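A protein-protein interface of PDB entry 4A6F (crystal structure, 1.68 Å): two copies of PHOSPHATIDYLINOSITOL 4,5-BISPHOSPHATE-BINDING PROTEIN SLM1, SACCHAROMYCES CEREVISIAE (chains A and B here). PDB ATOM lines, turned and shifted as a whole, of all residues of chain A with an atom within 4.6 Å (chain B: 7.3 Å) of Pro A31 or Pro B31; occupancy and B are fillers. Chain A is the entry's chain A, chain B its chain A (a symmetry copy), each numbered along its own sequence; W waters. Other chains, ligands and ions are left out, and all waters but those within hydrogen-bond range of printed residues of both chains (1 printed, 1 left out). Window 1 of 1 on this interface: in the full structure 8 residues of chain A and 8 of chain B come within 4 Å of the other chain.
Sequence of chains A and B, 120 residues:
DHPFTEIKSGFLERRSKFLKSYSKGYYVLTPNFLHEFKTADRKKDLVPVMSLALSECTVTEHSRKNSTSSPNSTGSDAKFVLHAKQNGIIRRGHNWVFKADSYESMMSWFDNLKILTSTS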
ATOM      1  N   THR A   5      -8.498  15.616  20.105  1.00  0.00           N
ATOM      2  CA  THR A   5      -8.756  14.232  20.481  1.00  0.00           C
ATOM      3  C   THR A   5      -7.578  13.764  21.329  1.00  0.00           C
ATOM      4  O   THR A   5      -7.012  12.691  21.105  1.00  0.00           O
ATOM      5  CB  THR A   5      -9.028  13.285  19.298  1.00  0.00           C
ATOM      6  OG1 THR A   5      -7.791  12.829  18.734  1.00  0.00           O
ATOM      7  CG2 THR A   5      -9.903  13.974  18.244  1.00  0.00           C
ATOM      8  N   ILE A   7      -5.760  12.165  24.376  1.00  0.00           N
ATOM      9  CA  ILE A   7      -6.008  11.133  25.372  1.00  0.00           C
ATOM     10  C   ILE A   7      -5.313  11.495  26.681  1.00  0.00           C
ATOM     11  O   ILE A   7      -5.874  11.342  27.766  1.00  0.00           O
ATOM     12  CB  ILE A   7      -5.520   9.758  24.874  1.00  0.00           C
ATOM     13  CG1 ILE A   7      -6.278   9.359  23.614  1.00  0.00           C
ATOM     14  CG2 ILE A   7      -5.676   8.686  25.956  1.00  0.00           C
ATOM     15  CD1 ILE A   7      -5.704   8.172  22.940  1.00  0.00           C
ATOM     16  N   THR A  30      -2.258  11.229  21.326  1.00  0.00           N
ATOM     17  CA  THR A  30      -3.501  11.047  20.570  1.00  0.00           C
ATOM     18  C   THR A  30      -3.584   9.576  20.171  1.00  0.00           C
ATOM     19  O   THR A  30      -2.684   8.812  20.477  1.00  0.00           O
ATOM     20  CB  THR A  30      -3.531  11.913  19.301  1.00  0.00           C
ATOM     21  OG1 THR A  30      -2.568  11.402  18.374  1.00  0.00           O
ATOM     22  CG2 THR A  30      -3.219  13.346  19.635  1.00  0.00           C
ATOM     23  N   PRO A  31      -4.667   9.165  19.486  1.00  0.00           N
ATOM     24  CA  PRO A  31      -4.683   7.761  19.056  1.00  0.00           C
ATOM     25  C   PRO A  31      -3.622   7.423  18.013  1.00  0.00           C
ATOM     26  O   PRO A  31      -3.350   6.246  17.797  1.00  0.00           O
ATOM     27  CB  PRO A  31      -6.084   7.594  18.461  1.00  0.00           C
ATOM     28  CG  PRO A  31      -6.915   8.628  19.153  1.00  0.00           C
ATOM     29  CD  PRO A  31      -5.985   9.808  19.328  1.00  0.00           C
ATOM     30  N   ASN A  32      -3.010   8.433  17.401  1.00  0.00           N
ATOM     31  CA  ASN A  32      -2.050   8.187  16.331  1.00  0.00           C
ATOM     32  C   ASN A  32      -0.596   8.468  16.704  1.00  0.00           C
ATOM     33  O   ASN A  32       0.297   7.782  16.229  1.00  0.00           O
ATOM     34  CB  ASN A  32      -2.415   8.999  15.093  1.00  0.00           C
ATOM     35  CG  ASN A  32      -3.679   8.503  14.435  1.00  0.00           C
ATOM     36  OD1 ASN A  32      -4.003   7.321  14.511  1.00  0.00           O
ATOM     37  ND2 ASN A  32      -4.389   9.397  13.775  1.00  0.00           N
ATOM     38  N   PHE A  33      -0.371   9.479  17.540  1.00  0.00           N
ATOM     39  CA  PHE A  33       0.989   9.955  17.824  1.00  0.00           C
ATOM     40  C   PHE A  33       1.209  10.296  19.288  1.00  0.00           C
ATOM     41  O   PHE A  33       0.269  10.619  20.020  1.00  0.00           O
ATOM     42  CB  PHE A  33       1.279  11.253  17.067  1.00  0.00           C
ATOM     43  CG  PHE A  33       1.404  11.095  15.582  1.00  0.00           C
ATOM     44  CD1 PHE A  33       2.577  10.633  15.014  1.00  0.00           C
ATOM     45  CD2 PHE A  33       0.358  11.453  14.753  1.00  0.00           C
ATOM     46  CE1 PHE A  33       2.692  10.503  13.639  1.00  0.00           C
ATOM     47  CE2 PHE A  33       0.465  11.328  13.375  1.00  0.00           C
ATOM     48  CZ  PHE A  33       1.638  10.857  12.820  1.00  0.00           C
ATOM     49  N   LEU A  54       2.647   6.013  16.809  1.00  0.00           N
ATOM     50  CA  LEU A  54       2.403   4.946  17.769  1.00  0.00           C
ATOM     51  C   LEU A  54       2.392   3.567  17.101  1.00  0.00           C
ATOM     52  O   LEU A  54       2.665   2.556  17.740  1.00  0.00           O
ATOM     53  CB  LEU A  54       1.086   5.187  18.512  1.00  0.00           C
ATOM     54  CG  LEU A  54       1.037   6.493  19.314  1.00  0.00           C
ATOM     55  CD1 LEU A  54      -0.311   6.659  20.022  1.00  0.00           C
ATOM     56  CD2 LEU A  54       2.179   6.538  20.303  1.00  0.00           C
ATOM     57  N   LEU A 116      -2.352   1.719  23.329  1.00  0.00           N
ATOM     58  CA  LEU A 116      -2.385   2.276  21.985  1.00  0.00           C
ATOM     59  C   LEU A 116      -1.299   1.688  21.090  1.00  0.00           C
ATOM     60  O   LEU A 116      -1.197   2.049  19.913  1.00  0.00           O
ATOM     61  CB  LEU A 116      -2.259   3.807  22.030  1.00  0.00           C
ATOM     62  CG  LEU A 116      -3.468   4.585  22.560  1.00  0.00           C
ATOM     63  CD1 LEU A 116      -3.108   6.053  22.815  1.00  0.00           C
ATOM     64  CD2 LEU A 116      -4.664   4.468  21.619  1.00  0.00           C
ATOM     65  N   THR B   5      -8.713   5.405  26.415  1.00  0.00           N
ATOM     66  CA  THR B   5      -8.483   6.353  25.333  1.00  0.00           C
ATOM     67  C   THR B   5      -9.627   7.361  25.361  1.00  0.00           C
ATOM     68  O   THR B   5     -10.242   7.662  24.335  1.00  0.00           O
ATOM     69  CB  THR B   5      -8.312   5.712  23.943  1.00  0.00           C
ATOM     70  OG1 THR B   5      -9.595   5.456  23.355  1.00  0.00           O
ATOM     71  CG2 THR B   5      -7.475   4.431  24.037  1.00  0.00           C
ATOM     72  N   GLU B   6      -9.906   7.884  26.552  1.00  0.00           N
ATOM     73  CA  GLU B   6     -10.974   8.864  26.697  1.00  0.00           C
ATOM     74  C   GLU B   6     -10.489  10.214  26.205  1.00  0.00           C
ATOM     75  O   GLU B   6      -9.377  10.650  26.538  1.00  0.00           O
ATOM     76  CB  GLU B   6     -11.423   8.964  28.152  1.00  0.00           C
ATOM     77  CG  GLU B   6     -11.601  10.390  28.639  1.00  0.00           C
ATOM     78  CD  GLU B   6     -11.941  10.456  30.101  1.00  0.00           C
ATOM     79  OE1 GLU B   6     -12.437   9.439  30.641  1.00  0.00           O
ATOM     80  OE2 GLU B   6     -11.720  11.524  30.708  1.00  0.00           O
ATOM     81  N   ILE B   7     -11.323  10.863  25.398  1.00  0.00           N
ATOM     82  CA  ILE B   7     -11.054  12.207  24.907  1.00  0.00           C
ATOM     83  C   ILE B   7     -11.661  13.239  25.855  1.00  0.00           C
ATOM     84  O   ILE B   7     -11.045  14.256  26.172  1.00  0.00           O
ATOM     85  CB  ILE B   7     -11.618  12.398  23.486  1.00  0.00           C
ATOM     86  CG1 ILE B   7     -10.948  11.425  22.523  1.00  0.00           C
ATOM     87  CG2 ILE B   7     -11.439  13.840  23.003  1.00  0.00           C
ATOM     88  CD1 ILE B   7     -11.601  11.376  21.195  1.00  0.00           C
ATOM     89  N   LEU B  29     -16.429  10.242  26.172  1.00  0.00           N
ATOM     90  CA  LEU B  29     -16.240  10.329  24.730  1.00  0.00           C
ATOM     91  C   LEU B  29     -14.934   9.652  24.308  1.00  0.00           C
ATOM     92  O   LEU B  29     -13.864  10.003  24.792  1.00  0.00           O
ATOM     93  CB  LEU B  29     -16.222  11.802  24.316  1.00  0.00           C
ATOM     94  CG  LEU B  29     -16.029  12.109  22.833  1.00  0.00           C
ATOM     95  CD1 LEU B  29     -17.171  11.534  21.975  1.00  0.00           C
ATOM     96  CD2 LEU B  29     -15.938  13.618  22.649  1.00  0.00           C
ATOM     97  N   THR B  30     -15.024   8.683  23.400  1.00  0.00           N
ATOM     98  CA  THR B  30     -13.833   8.047  22.828  1.00  0.00           C
ATOM     99  C   THR B  30     -13.825   8.348  21.332  1.00  0.00           C
ATOM    100  O   THR B  30     -14.732   8.996  20.838  1.00  0.00           O
ATOM    101  CB  THR B  30     -13.845   6.524  23.033  1.00  0.00           C
ATOM    102  OG1 THR B  30     -14.876   5.959  22.218  1.00  0.00           O
ATOM    103  CG2 THR B  30     -14.087   6.190  24.479  1.00  0.00           C
ATOM    104  N   PRO B  31     -12.798   7.883  20.597  1.00  0.00           N
ATOM    105  CA  PRO B  31     -12.855   8.129  19.151  1.00  0.00           C
ATOM    106  C   PRO B  31     -13.986   7.387  18.443  1.00  0.00           C
ATOM    107  O   PRO B  31     -14.311   7.732  17.312  1.00  0.00           O
ATOM    108  CB  PRO B  31     -11.497   7.623  18.656  1.00  0.00           C
ATOM    109  CG  PRO B  31     -10.592   7.748  19.841  1.00  0.00           C
ATOM    110  CD  PRO B  31     -11.468   7.407  21.025  1.00  0.00           C
ATOM    111  N   ASN B  32     -14.595   6.409  19.107  1.00  0.00           N
ATOM    112  CA  ASN B  32     -15.623   5.597  18.464  1.00  0.00           C
ATOM    113  C   ASN B  32     -17.042   5.855  18.965  1.00  0.00           C
ATOM    114  O   ASN B  32     -17.984   5.771  18.191  1.00  0.00           O
ATOM    115  CB  ASN B  32     -15.301   4.115  18.615  1.00  0.00           C
ATOM    116  CG  ASN B  32     -14.095   3.706  17.806  1.00  0.00           C
ATOM    117  OD1 ASN B  32     -13.808   4.292  16.766  1.00  0.00           O
ATOM    118  ND2 ASN B  32     -13.392   2.689  18.269  1.00  0.00           N
ATOM    119  N   PHE B  33     -17.184   6.156  20.253  1.00  0.00           N
ATOM    120  CA  PHE B  33     -18.508   6.243  20.883  1.00  0.00           C
ATOM    121  C   PHE B  33     -18.632   7.405  21.853  1.00  0.00           C
ATOM    122  O   PHE B  33     -17.640   7.881  22.415  1.00  0.00           O
ATOM    123  CB  PHE B  33     -18.795   4.995  21.720  1.00  0.00           C
ATOM    124  CG  PHE B  33     -19.010   3.744  20.923  1.00  0.00           C
ATOM    125  CD1 PHE B  33     -20.229   3.486  20.323  1.00  0.00           C
ATOM    126  CD2 PHE B  33     -18.000   2.807  20.812  1.00  0.00           C
ATOM    127  CE1 PHE B  33     -20.427   2.320  19.599  1.00  0.00           C
ATOM    128  CE2 PHE B  33     -18.190   1.636  20.091  1.00  0.00           C
ATOM    129  CZ  PHE B  33     -19.409   1.394  19.489  1.00  0.00           C
ATOM    130  N   LEU B  34     -19.872   7.834  22.066  1.00  0.00           N
ATOM    131  CA  LEU B  34     -20.220   8.575  23.268  1.00  0.00           C
ATOM    132  C   LEU B  34     -20.904   7.562  24.169  1.00  0.00           C
ATOM    133  O   LEU B  34     -21.991   7.077  23.847  1.00  0.00           O
ATOM    134  CB  LEU B  34     -21.168   9.737  22.948  1.00  0.00           C
ATOM    135  CG  LEU B  34     -21.627  10.550  24.175  1.00  0.00           C
ATOM    136  CD1 LEU B  34     -20.495  11.312  24.845  1.00  0.00           C
ATOM    137  CD2 LEU B  34     -22.711  11.549  23.739  1.00  0.00           C
ATOM    138  N   LEU B  54     -20.359   7.166  17.004  1.00  0.00           N
ATOM    139  CA  LEU B  54     -20.098   8.493  16.466  1.00  0.00           C
ATOM    140  C   LEU B  54     -20.174   8.516  14.936  1.00  0.00           C
ATOM    141  O   LEU B  54     -20.445   9.550  14.334  1.00  0.00           O
ATOM    142  CB  LEU B  54     -18.733   9.002  16.938  1.00  0.00           C
ATOM    143  CG  LEU B  54     -18.593   9.130  18.459  1.00  0.00           C
ATOM    144  CD1 LEU B  54     -17.201   9.640  18.848  1.00  0.00           C
ATOM    145  CD2 LEU B  54     -19.674  10.033  19.008  1.00  0.00           C
ATOM    146  N   SER B  55     -19.931   7.364  14.316  1.00  0.00           N
ATOM    147  CA  SER B  55     -19.885   7.292  12.853  1.00  0.00           C
ATOM    148  C   SER B  55     -21.218   7.660  12.207  1.00  0.00           C
ATOM    149  O   SER B  55     -21.261   8.061  11.043  1.00  0.00           O
ATOM    150  CB  SER B  55     -19.447   5.905  12.391  1.00  0.00           C
ATOM    151  OG  SER B  55     -20.364   4.920  12.819  1.00  0.00           O
ATOM    152  N   LEU B 116     -15.150  14.739  15.798  1.00  0.00           N
ATOM    153  CA  LEU B 116     -15.174  13.288  15.693  1.00  0.00           C
ATOM    154  C   LEU B 116     -16.329  12.791  14.830  1.00  0.00           C
ATOM    155  O   LEU B 116     -16.486  11.582  14.633  1.00  0.00           O
ATOM    156  CB  LEU B 116     -15.244  12.644  17.087  1.00  0.00           C
ATOM    157  CG  LEU B 116     -13.980  12.726  17.950  1.00  0.00           C
ATOM    158  CD1 LEU B 116     -14.273  12.307  19.395  1.00  0.00           C
ATOM    159  CD2 LEU B 116     -12.844  11.896  17.357  1.00  0.00           C
ATOM    160  N   THR B 117     -17.127  13.720  14.304  1.00  0.00           N
ATOM    161  CA  THR B 117     -18.332  13.344  13.558  1.00  0.00           C
ATOM    162  C   THR B 117     -18.456  14.051  12.206  1.00  0.00           C
ATOM    163  O   THR B 117     -19.560  14.184  11.667  1.00  0.00           O
ATOM    164  CB  THR B 117     -19.626  13.615  14.384  1.00  0.00           C
ATOM    165  OG1 THR B 117     -19.642  14.978  14.824  1.00  0.00           O
ATOM    166  CG2 THR B 117     -19.702  12.705  15.615  1.00  0.00           C
HETATM  167  O   HOH W   1      -7.833   8.869  28.950  1.00  0.00           O
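Water W1 lies within hydrogen-bond range of N of Glu B6 and O of Ile A7.
Along chain A the printed residues that touch a printed residue of chain B span positions 5 to 116. Among the printed residues, no Asp or Glu carboxylate lies within 4 Å of a Lys or Arg side-chain nitrogen of the other chain.
Pro A31 touches one residue of chain B. Of the printed residues of chain B, Leu A116 touches Thr B5. Printed residues of chain A within 4 Å of Glu B6: Ile A7 (3.6 Å). Of the printed residues of chain A, Thr B5 touches Ile A7 and Leu A116. Printed residues of chain A within 4 Å of Leu B116: Thr A5 (3.7 Å). Phe A33 touches none of the printed residues of chain B. The nearest printed residue of chain B that does not touch Pro A31 is Thr B5 (5.8 Å). The nearest printed residue of chain A that does not touch Thr B5 is Pro A31 (5.8 Å).
N of Ile B7 sits at hydrogen-bond distance from O of Leu B29.
Thr A5 touches Ile B7, and with the chains exchanged Ile A7 touches Thr B5. Thr A5 touches Leu B116, and with the chains exchanged Leu A116 touches Thr B5. Pro B31 touches its own counterpart, Pro A31.
Thr A5 touches Ile B7 (CA to CG2, 3.7 Å). Thr A5 touches Leu B116 (CG2 to CD2, 3.7 Å). Ile A7 touches Thr B5. CA of Ile A7 touches O of Glu B6, at 3.6 Å. Pro A31 touches Pro B31. CG2 of Thr B5 touches CD2 of Leu A116, 3.7 Å away.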
